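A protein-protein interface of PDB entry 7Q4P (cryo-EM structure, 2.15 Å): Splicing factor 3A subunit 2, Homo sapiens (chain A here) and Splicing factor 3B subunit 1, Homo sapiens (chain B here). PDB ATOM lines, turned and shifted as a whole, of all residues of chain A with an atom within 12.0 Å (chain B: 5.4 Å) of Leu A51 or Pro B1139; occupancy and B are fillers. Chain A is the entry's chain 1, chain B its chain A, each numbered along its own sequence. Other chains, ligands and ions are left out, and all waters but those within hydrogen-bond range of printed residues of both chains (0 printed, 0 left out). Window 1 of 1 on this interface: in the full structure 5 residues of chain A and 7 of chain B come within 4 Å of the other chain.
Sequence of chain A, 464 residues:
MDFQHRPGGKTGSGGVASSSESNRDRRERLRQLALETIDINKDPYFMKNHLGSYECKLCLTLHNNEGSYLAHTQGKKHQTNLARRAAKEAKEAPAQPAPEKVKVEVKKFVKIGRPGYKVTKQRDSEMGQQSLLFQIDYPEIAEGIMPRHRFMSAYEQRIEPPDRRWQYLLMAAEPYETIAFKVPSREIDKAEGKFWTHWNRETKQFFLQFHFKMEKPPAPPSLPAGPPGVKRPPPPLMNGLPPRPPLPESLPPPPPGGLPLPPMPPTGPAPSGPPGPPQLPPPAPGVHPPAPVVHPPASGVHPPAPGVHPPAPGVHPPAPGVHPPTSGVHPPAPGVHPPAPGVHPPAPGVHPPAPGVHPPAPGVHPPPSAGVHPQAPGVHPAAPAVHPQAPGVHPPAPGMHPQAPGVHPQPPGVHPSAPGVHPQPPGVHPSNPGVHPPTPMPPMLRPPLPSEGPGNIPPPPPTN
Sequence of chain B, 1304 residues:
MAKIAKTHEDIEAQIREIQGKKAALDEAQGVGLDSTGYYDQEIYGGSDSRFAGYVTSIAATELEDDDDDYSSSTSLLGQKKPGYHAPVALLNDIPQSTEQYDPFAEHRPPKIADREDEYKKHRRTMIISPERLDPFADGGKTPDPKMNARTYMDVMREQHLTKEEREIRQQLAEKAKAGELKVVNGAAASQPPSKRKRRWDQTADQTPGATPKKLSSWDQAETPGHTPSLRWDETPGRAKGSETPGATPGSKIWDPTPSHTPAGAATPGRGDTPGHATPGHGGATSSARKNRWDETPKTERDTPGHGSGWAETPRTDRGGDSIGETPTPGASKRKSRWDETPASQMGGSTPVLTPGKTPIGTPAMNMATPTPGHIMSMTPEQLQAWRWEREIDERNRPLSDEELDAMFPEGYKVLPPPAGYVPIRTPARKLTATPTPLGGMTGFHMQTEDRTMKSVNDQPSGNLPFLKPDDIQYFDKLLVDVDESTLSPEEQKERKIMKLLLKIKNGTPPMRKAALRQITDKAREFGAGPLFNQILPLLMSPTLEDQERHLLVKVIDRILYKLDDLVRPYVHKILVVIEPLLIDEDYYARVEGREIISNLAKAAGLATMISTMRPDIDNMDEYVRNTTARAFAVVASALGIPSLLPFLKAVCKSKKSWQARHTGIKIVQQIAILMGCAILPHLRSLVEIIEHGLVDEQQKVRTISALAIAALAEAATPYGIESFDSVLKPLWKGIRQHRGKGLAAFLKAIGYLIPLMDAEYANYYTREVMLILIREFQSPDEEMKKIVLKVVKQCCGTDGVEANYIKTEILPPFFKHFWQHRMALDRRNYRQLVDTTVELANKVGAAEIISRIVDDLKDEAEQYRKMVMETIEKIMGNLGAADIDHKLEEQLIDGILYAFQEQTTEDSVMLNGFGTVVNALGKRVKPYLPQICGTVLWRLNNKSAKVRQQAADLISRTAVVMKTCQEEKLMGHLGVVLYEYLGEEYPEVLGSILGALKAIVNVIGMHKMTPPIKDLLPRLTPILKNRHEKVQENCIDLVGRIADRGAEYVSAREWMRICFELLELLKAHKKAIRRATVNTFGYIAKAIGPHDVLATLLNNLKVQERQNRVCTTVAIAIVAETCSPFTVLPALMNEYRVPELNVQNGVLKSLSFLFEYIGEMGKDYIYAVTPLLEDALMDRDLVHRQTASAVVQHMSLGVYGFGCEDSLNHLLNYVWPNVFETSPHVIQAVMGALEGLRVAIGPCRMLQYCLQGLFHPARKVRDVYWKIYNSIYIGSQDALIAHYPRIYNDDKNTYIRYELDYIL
The side-chain amide nitrogen (NE2) of Gln B1144 lies within hydrogen-bond range of the backbone carbonyl oxygen (O) of His A50 (2.9 Å).
OD2 of Asp B1179 lies within hydrogen-bond range of NE2 of His A50, 3.3 Å away.
N of Leu B1141 is in hydrogen-bond range of O of Leu A51.
N of Gly A52 lies close to O of Pro B1139 (3.4 Å).
The side-chain carboxylate of Glu A55 lies within salt-bridge range of the guanidinium group of Arg B1180 (3.0 Å).
The backbone carbonyl oxygen of Met A47 sits at hydrogen-bond distance from the backbone NH of Glu A55, 2.9 Å away.
The backbone NH (N) of Leu A51 sits close to the side-chain amide oxygen (OD1) of Asn A49 (3.1 Å).
The side-chain amide oxygen (OD1) of Asn A49 is in hydrogen-bond range of the backbone NH (N) of Gly A52 (3.0 Å).
The backbone carbonyl oxygen (O) of Val B1138 is in hydrogen-bond range of the side-chain amide nitrogen (NE2) of Gln B1144, 2.8 Å away.
A ring nitrogen (NE2) of His B1184 sits close to the side-chain carboxylate (OD2) of Asp B1179, at 3.4 Å.
ND1 of His B1184 lies within hydrogen-bond range of OD2 of Asp B1181 (3.1 Å).
Among the printed residues, pairs that only touch across the chains: His A50 with Pro B1139 (3.0 Å), His A50 with Glu B1140 (3.7 Å), Leu A51 with Pro B1139 (3.7 Å), Leu A51 with Glu B1140 (3.5 Å), Leu A51 with Arg B1180 (3.7 Å), Leu A51 with His B1184 (3.5 Å) and Leu A62 with Arg B1180 (3.5 Å).
Asn A49 touches none of the printed residues of chain B.
Of the printed residues of chain B, His A50 touches Pro B1139, Glu B1140, Gln B1144 and Asp B1179.
Of chain B, only Pro B1139, Glu B1140, Leu B1141, Arg B1180 and His B1184 come within 4 Å of Leu A51.
Of the printed residues of chain B, Glu A55 touches Arg B1180.
Of the printed residues of chain B, Leu A62 touches Arg B1180 (3.5 Å).
Glu A66 touches none of the printed residues of chain B.
Of chain A, only His A50, Leu A51 and Gly A52 come within 4 Å of Pro B1139.
Glu B1140 touches just these residues of chain A: His A50 and Leu A51.
Printed residues of chain A within 4 Å of Leu B1141: Leu A51.
Arg B1180 touches just these residues of chain A: Leu A51, Glu A55 and Leu A62.
Asp B1181 touches none of the printed residues of chain A.
Of the printed residues of chain A, His B1184 touches Leu A51.
The nearest residue of chain A that does not touch Pro B1139 is Asn A49 (4.5 Å).
Printed residues of chain B that touch a printed residue of chain A: Pro B1139, Glu B1140, Leu B1141, Gln B1144, Asp B1179, Arg B1180 and His B1184.
Hydrophobic or aromatic side chains of chain A within 4 Å of the printed part of chain B: His A50, Leu A51 and Leu A62.
Among the printed residues, 12 pairs touch across the chains.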
ATOM      1  N   PHE A  46      14.348   9.006  35.536  1.00  0.00           N
ATOM      2  CA  PHE A  46      13.615   9.253  34.311  1.00  0.00           C
ATOM      3  C   PHE A  46      14.026  10.607  33.748  1.00  0.00           C
ATOM      4  O   PHE A  46      13.933  11.639  34.420  1.00  0.00           O
ATOM      5  CB  PHE A  46      12.123   9.249  34.636  1.00  0.00           C
ATOM      6  CG  PHE A  46      11.198   9.280  33.455  1.00  0.00           C
ATOM      7  CD1 PHE A  46      10.969   8.135  32.709  1.00  0.00           C
ATOM      8  CD2 PHE A  46      10.502  10.436  33.135  1.00  0.00           C
ATOM      9  CE1 PHE A  46      10.081   8.151  31.647  1.00  0.00           C
ATOM     10  CE2 PHE A  46       9.625  10.455  32.063  1.00  0.00           C
ATOM     11  CZ  PHE A  46       9.406   9.310  31.330  1.00  0.00           C
ATOM     12  N   MET A  47      14.507  10.557  32.511  1.00  0.00           N
ATOM     13  CA  MET A  47      14.928  11.741  31.782  1.00  0.00           C
ATOM     14  C   MET A  47      14.473  11.608  30.335  1.00  0.00           C
ATOM     15  O   MET A  47      14.451  10.508  29.785  1.00  0.00           O
ATOM     16  CB  MET A  47      16.446  11.947  31.837  1.00  0.00           C
ATOM     17  CG  MET A  47      17.259  10.719  31.475  1.00  0.00           C
ATOM     18  SD  MET A  47      18.942  11.161  30.974  1.00  0.00           S
ATOM     19  CE  MET A  47      18.676  11.637  29.266  1.00  0.00           C
ATOM     20  N   LYS A  48      14.092  12.750  29.755  1.00  0.00           N
ATOM     21  CA  LYS A  48      13.807  12.877  28.337  1.00  0.00           C
ATOM     22  C   LYS A  48      15.080  13.337  27.631  1.00  0.00           C
ATOM     23  O   LYS A  48      15.667  14.354  28.005  1.00  0.00           O
ATOM     24  CB  LYS A  48      12.631  13.841  28.144  1.00  0.00           C
ATOM     25  CG  LYS A  48      11.980  13.832  26.769  1.00  0.00           C
ATOM     26  CD  LYS A  48      10.746  14.711  26.699  1.00  0.00           C
ATOM     27  CE  LYS A  48      10.029  14.652  25.364  1.00  0.00           C
ATOM     28  NZ  LYS A  48       8.778  15.450  25.367  1.00  0.00           N
ATOM     29  N   ASN A  49      15.508  12.564  26.618  1.00  0.00           N
ATOM     30  CA  ASN A  49      16.653  12.904  25.784  1.00  0.00           C
ATOM     31  C   ASN A  49      16.266  13.972  24.756  1.00  0.00           C
ATOM     32  O   ASN A  49      15.098  14.336  24.624  1.00  0.00           O
ATOM     33  CB  ASN A  49      17.297  11.673  25.123  1.00  0.00           C
ATOM     34  CG  ASN A  49      16.330  10.770  24.378  1.00  0.00           C
ATOM     35  OD1 ASN A  49      15.528  11.232  23.566  1.00  0.00           O
ATOM     36  ND2 ASN A  49      16.392   9.473  24.644  1.00  0.00           N
ATOM     37  N   HIS A  50      17.271  14.442  24.002  1.00  0.00           N
ATOM     38  CA  HIS A  50      17.127  15.472  22.981  1.00  0.00           C
ATOM     39  C   HIS A  50      16.435  14.926  21.726  1.00  0.00           C
ATOM     40  O   HIS A  50      16.157  15.668  20.789  1.00  0.00           O
ATOM     41  CB  HIS A  50      18.499  16.104  22.683  1.00  0.00           C
ATOM     42  CG  HIS A  50      19.483  15.126  22.136  1.00  0.00           C
ATOM     43  ND1 HIS A  50      20.138  14.210  22.938  1.00  0.00           N
ATOM     44  CD2 HIS A  50      19.898  14.893  20.872  1.00  0.00           C
ATOM     45  CE1 HIS A  50      20.927  13.464  22.195  1.00  0.00           C
ATOM     46  NE2 HIS A  50      20.804  13.868  20.924  1.00  0.00           N
ATOM     47  N   LEU A  51      16.173  13.614  21.702  1.00  0.00           N
ATOM     48  CA  LEU A  51      15.532  12.965  20.572  1.00  0.00           C
ATOM     49  C   LEU A  51      14.048  12.802  20.873  1.00  0.00           C
ATOM     50  O   LEU A  51      13.271  12.402  20.008  1.00  0.00           O
ATOM     51  CB  LEU A  51      16.182  11.598  20.328  1.00  0.00           C
ATOM     52  CG  LEU A  51      17.671  11.603  19.989  1.00  0.00           C
ATOM     53  CD1 LEU A  51      18.269  10.208  20.138  1.00  0.00           C
ATOM     54  CD2 LEU A  51      17.923  12.147  18.590  1.00  0.00           C
ATOM     55  N   GLY A  52      13.672  13.067  22.129  1.00  0.00           N
ATOM     56  CA  GLY A  52      12.279  12.962  22.523  1.00  0.00           C
ATOM     57  C   GLY A  52      11.942  11.644  23.213  1.00  0.00           C
ATOM     58  O   GLY A  52      10.896  11.555  23.844  1.00  0.00           O
ATOM     59  N   SER A  53      12.818  10.636  23.096  1.00  0.00           N
ATOM     60  CA  SER A  53      12.668   9.372  23.805  1.00  0.00           C
ATOM     61  C   SER A  53      13.089   9.535  25.265  1.00  0.00           C
ATOM     62  O   SER A  53      13.502  10.611  25.712  1.00  0.00           O
ATOM     63  CB  SER A  53      13.447   8.276  23.121  1.00  0.00           C
ATOM     64  OG  SER A  53      12.886   7.991  21.854  1.00  0.00           O
ATOM     65  N   TYR A  54      12.958   8.439  26.014  1.00  0.00           N
ATOM     66  CA  TYR A  54      13.192   8.471  27.444  1.00  0.00           C
ATOM     67  C   TYR A  54      14.305   7.492  27.799  1.00  0.00           C
ATOM     68  O   TYR A  54      14.483   6.467  27.146  1.00  0.00           O
ATOM     69  CB  TYR A  54      11.880   8.213  28.189  1.00  0.00           C
ATOM     70  CG  TYR A  54      10.750   9.147  27.830  1.00  0.00           C
ATOM     71  CD1 TYR A  54      10.707  10.436  28.340  1.00  0.00           C
ATOM     72  CD2 TYR A  54       9.705   8.744  27.006  1.00  0.00           C
ATOM     73  CE1 TYR A  54       9.669  11.304  28.033  1.00  0.00           C
ATOM     74  CE2 TYR A  54       8.654   9.596  26.693  1.00  0.00           C
ATOM     75  CZ  TYR A  54       8.640  10.886  27.201  1.00  0.00           C
ATOM     76  OH  TYR A  54       7.614  11.733  26.885  1.00  0.00           O
ATOM     77  N   GLU A  55      15.049   7.835  28.848  1.00  0.00           N
ATOM     78  CA  GLU A  55      16.187   7.055  29.308  1.00  0.00           C
ATOM     79  C   GLU A  55      16.063   6.828  30.811  1.00  0.00           C
ATOM     80  O   GLU A  55      15.507   7.659  31.527  1.00  0.00           O
ATOM     81  CB  GLU A  55      17.473   7.837  29.041  1.00  0.00           C
ATOM     82  CG  GLU A  55      17.713   8.131  27.571  1.00  0.00           C
ATOM     83  CD  GLU A  55      19.150   8.485  27.226  1.00  0.00           C
ATOM     84  OE1 GLU A  55      20.044   7.697  27.583  1.00  0.00           O
ATOM     85  OE2 GLU A  55      19.373   9.545  26.612  1.00  0.00           O
ATOM     86  N   THR A  61      19.362   2.639  29.983  1.00  0.00           N
ATOM     87  CA  THR A  61      18.516   1.859  29.104  1.00  0.00           C
ATOM     88  C   THR A  61      17.595   2.830  28.388  1.00  0.00           C
ATOM     89  O   THR A  61      17.097   3.775  28.988  1.00  0.00           O
ATOM     90  CB  THR A  61      17.707   0.805  29.875  1.00  0.00           C
ATOM     91  OG1 THR A  61      17.137   1.376  31.053  1.00  0.00           O
ATOM     92  CG2 THR A  61      18.530  -0.409  30.251  1.00  0.00           C
ATOM     93  N   LEU A  62      17.313   2.552  27.121  1.00  0.00           N
ATOM     94  CA  LEU A  62      16.528   3.485  26.332  1.00  0.00           C
ATOM     95  C   LEU A  62      15.098   2.979  26.252  1.00  0.00           C
ATOM     96  O   LEU A  62      14.872   1.765  26.160  1.00  0.00           O
ATOM     97  CB  LEU A  62      17.113   3.589  24.924  1.00  0.00           C
ATOM     98  CG  LEU A  62      18.589   3.965  24.810  1.00  0.00           C
ATOM     99  CD1 LEU A  62      19.016   3.933  23.349  1.00  0.00           C
ATOM    100  CD2 LEU A  62      18.874   5.342  25.396  1.00  0.00           C
ATOM    101  N   HIS A  63      14.153   3.928  26.308  1.00  0.00           N
ATOM    102  CA  HIS A  63      12.723   3.648  26.291  1.00  0.00           C
ATOM    103  C   HIS A  63      12.016   4.562  25.293  1.00  0.00           C
ATOM    104  O   HIS A  63      12.297   5.756  25.243  1.00  0.00           O
ATOM    105  CB  HIS A  63      12.139   3.760  27.707  1.00  0.00           C
ATOM    106  CG  HIS A  63      12.976   3.050  28.717  1.00  0.00           C
ATOM    107  ND1 HIS A  63      13.029   1.660  28.800  1.00  0.00           N
ATOM    108  CD2 HIS A  63      13.835   3.527  29.649  1.00  0.00           C
ATOM    109  CE1 HIS A  63      13.894   1.318  29.736  1.00  0.00           C
ATOM    110  NE2 HIS A  63      14.403   2.443  30.270  1.00  0.00           N
ATOM    111  N   ASN A  64      11.125   3.970  24.494  1.00  0.00           N
ATOM    112  CA  ASN A  64      10.404   4.689  23.455  1.00  0.00           C
ATOM    113  C   ASN A  64       9.340   5.597  24.076  1.00  0.00           C
ATOM    114  O   ASN A  64       9.101   6.702  23.585  1.00  0.00           O
ATOM    115  CB  ASN A  64       9.793   3.722  22.440  1.00  0.00           C
ATOM    116  CG  ASN A  64      10.811   2.952  21.621  1.00  0.00           C
ATOM    117  OD1 ASN A  64      11.924   3.421  21.384  1.00  0.00           O
ATOM    118  ND2 ASN A  64      10.430   1.770  21.164  1.00  0.00           N
ATOM    119  N   ASN A  65       8.701   5.096  25.144  1.00  0.00           N
ATOM    120  CA  ASN A  65       7.604   5.765  25.823  1.00  0.00           C
ATOM    121  C   ASN A  65       7.742   5.578  27.335  1.00  0.00           C
ATOM    122  O   ASN A  65       8.708   4.976  27.804  1.00  0.00           O
ATOM    123  CB  ASN A  65       6.254   5.309  25.260  1.00  0.00           C
ATOM    124  CG  ASN A  65       6.112   3.804  25.163  1.00  0.00           C
ATOM    125  OD1 ASN A  65       6.061   3.115  26.178  1.00  0.00           O
ATOM    126  ND2 ASN A  65       5.989   3.287  23.950  1.00  0.00           N
ATOM    127  N   GLU A  66       6.767   6.117  28.083  1.00  0.00           N
ATOM    128  CA  GLU A  66       6.705   6.030  29.536  1.00  0.00           C
ATOM    129  C   GLU A  66       6.378   4.600  29.955  1.00  0.00           C
ATOM    130  O   GLU A  66       6.889   4.119  30.965  1.00  0.00           O
ATOM    131  CB  GLU A  66       5.638   6.973  30.096  1.00  0.00           C
ATOM    132  CG  GLU A  66       6.089   8.420  30.187  1.00  0.00           C
ATOM    133  CD  GLU A  66       5.902   9.286  28.949  1.00  0.00           C
ATOM    134  OE1 GLU A  66       6.015  10.522  29.081  1.00  0.00           O
ATOM    135  OE2 GLU A  66       5.648   8.732  27.858  1.00  0.00           O
ATOM    136  N   ARG B1137      17.021  22.299  16.832  1.00  0.00           N
ATOM    137  CA  ARG B1137      17.036  22.496  18.278  1.00  0.00           C
ATOM    138  C   ARG B1137      15.801  21.895  18.950  1.00  0.00           C
ATOM    139  O   ARG B1137      15.803  21.667  20.162  1.00  0.00           O
ATOM    140  CB  ARG B1137      17.071  23.991  18.606  1.00  0.00           C
ATOM    141  CG  ARG B1137      18.376  24.689  18.249  1.00  0.00           C
ATOM    142  CD  ARG B1137      18.324  26.199  18.451  1.00  0.00           C
ATOM    143  NE  ARG B1137      17.791  26.589  19.759  1.00  0.00           N
ATOM    144  CZ  ARG B1137      18.437  26.580  20.929  1.00  0.00           C
ATOM    145  NH1 ARG B1137      19.703  26.206  21.006  1.00  0.00           N
ATOM    146  NH2 ARG B1137      17.812  26.958  22.034  1.00  0.00           N
ATOM    147  N   VAL B1138      14.778  21.563  18.158  1.00  0.00           N
ATOM    148  CA  VAL B1138      13.574  20.909  18.655  1.00  0.00           C
ATOM    149  C   VAL B1138      13.915  19.484  19.093  1.00  0.00           C
ATOM    150  O   VAL B1138      14.464  18.703  18.327  1.00  0.00           O
ATOM    151  CB  VAL B1138      12.503  20.917  17.553  1.00  0.00           C
ATOM    152  CG1 VAL B1138      11.280  20.072  17.880  1.00  0.00           C
ATOM    153  CG2 VAL B1138      12.109  22.328  17.155  1.00  0.00           C
ATOM    154  N   PRO B1139      13.583  19.087  20.341  1.00  0.00           N
ATOM    155  CA  PRO B1139      13.945  17.764  20.854  1.00  0.00           C
ATOM    156  C   PRO B1139      12.998  16.658  20.393  1.00  0.00           C
ATOM    157  O   PRO B1139      12.301  16.052  21.205  1.00  0.00           O
ATOM    158  CB  PRO B1139      13.875  17.978  22.368  1.00  0.00           C
ATOM    159  CG  PRO B1139      12.805  19.039  22.557  1.00  0.00           C
ATOM    160  CD  PRO B1139      12.866  19.913  21.321  1.00  0.00           C
ATOM    161  N   GLU B1140      12.952  16.443  19.076  1.00  0.00           N
ATOM    162  CA  GLU B1140      12.189  15.378  18.449  1.00  0.00           C
ATOM    163  C   GLU B1140      13.054  14.712  17.385  1.00  0.00           C
ATOM    164  O   GLU B1140      13.949  15.329  16.811  1.00  0.00           O
ATOM    165  CB  GLU B1140      10.897  15.922  17.849  1.00  0.00           C
ATOM    166  CG  GLU B1140       9.816  16.135  18.887  1.00  0.00           C
ATOM    167  CD  GLU B1140       8.530  16.757  18.369  1.00  0.00           C
ATOM    168  OE1 GLU B1140       8.132  17.817  18.898  1.00  0.00           O
ATOM    169  OE2 GLU B1140       7.917  16.175  17.450  1.00  0.00           O
ATOM    170  N   LEU B1141      12.813  13.420  17.174  1.00  0.00           N
ATOM    171  CA  LEU B1141      13.676  12.640  16.315  1.00  0.00           C
ATOM    172  C   LEU B1141      13.348  12.941  14.865  1.00  0.00           C
ATOM    173  O   LEU B1141      14.246  13.112  14.042  1.00  0.00           O
ATOM    174  CB  LEU B1141      13.414  11.165  16.580  1.00  0.00           C
ATOM    175  CG  LEU B1141      14.417  10.227  15.916  1.00  0.00           C
ATOM    176  CD1 LEU B1141      15.655  10.104  16.772  1.00  0.00           C
ATOM    177  CD2 LEU B1141      13.787   8.867  15.653  1.00  0.00           C
ATOM    178  N   GLN B1144      14.445  16.520  13.764  1.00  0.00           N
ATOM    179  CA  GLN B1144      15.882  16.649  13.597  1.00  0.00           C
ATOM    180  C   GLN B1144      16.331  15.837  12.394  1.00  0.00           C
ATOM    181  O   GLN B1144      17.232  16.271  11.696  1.00  0.00           O
ATOM    182  CB  GLN B1144      16.586  16.122  14.830  1.00  0.00           C
ATOM    183  CG  GLN B1144      16.627  17.194  15.890  1.00  0.00           C
ATOM    184  CD  GLN B1144      17.259  16.701  17.160  1.00  0.00           C
ATOM    185  OE1 GLN B1144      18.382  16.208  17.153  1.00  0.00           O
ATOM    186  NE2 GLN B1144      16.616  16.964  18.285  1.00  0.00           N
ATOM    187  N   ASP B1179      25.922  11.994  16.957  1.00  0.00           N
ATOM    188  CA  ASP B1179      24.714  11.514  17.607  1.00  0.00           C
ATOM    189  C   ASP B1179      24.733   9.990  17.707  1.00  0.00           C
ATOM    190  O   ASP B1179      25.109   9.351  16.743  1.00  0.00           O
ATOM    191  CB  ASP B1179      23.451  11.958  16.864  1.00  0.00           C
ATOM    192  CG  ASP B1179      22.262  12.196  17.783  1.00  0.00           C
ATOM    193  OD1 ASP B1179      21.879  11.239  18.463  1.00  0.00           O
ATOM    194  OD2 ASP B1179      21.739  13.347  17.841  1.00  0.00           O
ATOM    195  N   ARG B1180      24.249   9.427  18.824  1.00  0.00           N
ATOM    196  CA  ARG B1180      23.986   8.012  19.011  1.00  0.00           C
ATOM    197  C   ARG B1180      23.026   7.447  17.964  1.00  0.00           C
ATOM    198  O   ARG B1180      23.230   6.349  17.462  1.00  0.00           O
ATOM    199  CB  ARG B1180      23.322   7.840  20.371  1.00  0.00           C
ATOM    200  CG  ARG B1180      23.090   6.383  20.730  1.00  0.00           C
ATOM    201  CD  ARG B1180      21.741   6.123  21.372  1.00  0.00           C
ATOM    202  NE  ARG B1180      21.541   6.938  22.572  1.00  0.00           N
ATOM    203  CZ  ARG B1180      20.391   7.492  22.960  1.00  0.00           C
ATOM    204  NH1 ARG B1180      20.342   8.216  24.068  1.00  0.00           N
ATOM    205  NH2 ARG B1180      19.291   7.326  22.244  1.00  0.00           N
ATOM    206  N   ASP B1181      21.956   8.184  17.657  1.00  0.00           N
ATOM    207  CA  ASP B1181      20.972   7.724  16.684  1.00  0.00           C
ATOM    208  C   ASP B1181      21.630   7.394  15.344  1.00  0.00           C
ATOM    209  O   ASP B1181      22.400   8.193  14.816  1.00  0.00           O
ATOM    210  CB  ASP B1181      19.890   8.784  16.437  1.00  0.00           C
ATOM    211  CG  ASP B1181      18.783   8.324  15.482  1.00  0.00           C
ATOM    212  OD1 ASP B1181      18.434   7.125  15.494  1.00  0.00           O
ATOM    213  OD2 ASP B1181      18.266   9.171  14.710  1.00  0.00           O
ATOM    214  N   HIS B1184      20.388   9.875  12.384  1.00  0.00           N
ATOM    215  CA  HIS B1184      21.101  11.130  12.380  1.00  0.00           C
ATOM    216  C   HIS B1184      22.437  10.987  11.676  1.00  0.00           C
ATOM    217  O   HIS B1184      22.866  11.953  11.084  1.00  0.00           O
ATOM    218  CB  HIS B1184      21.464  11.545  13.784  1.00  0.00           C
ATOM    219  CG  HIS B1184      20.489  12.426  14.433  1.00  0.00           C
ATOM    220  ND1 HIS B1184      19.168  12.090  14.594  1.00  0.00           N
ATOM    221  CD2 HIS B1184      20.635  13.668  14.910  1.00  0.00           C
ATOM    222  CE1 HIS B1184      18.557  13.066  15.230  1.00  0.00           C
ATOM    223  NE2 HIS B1184      19.442  14.033  15.433  1.00  0.00           N
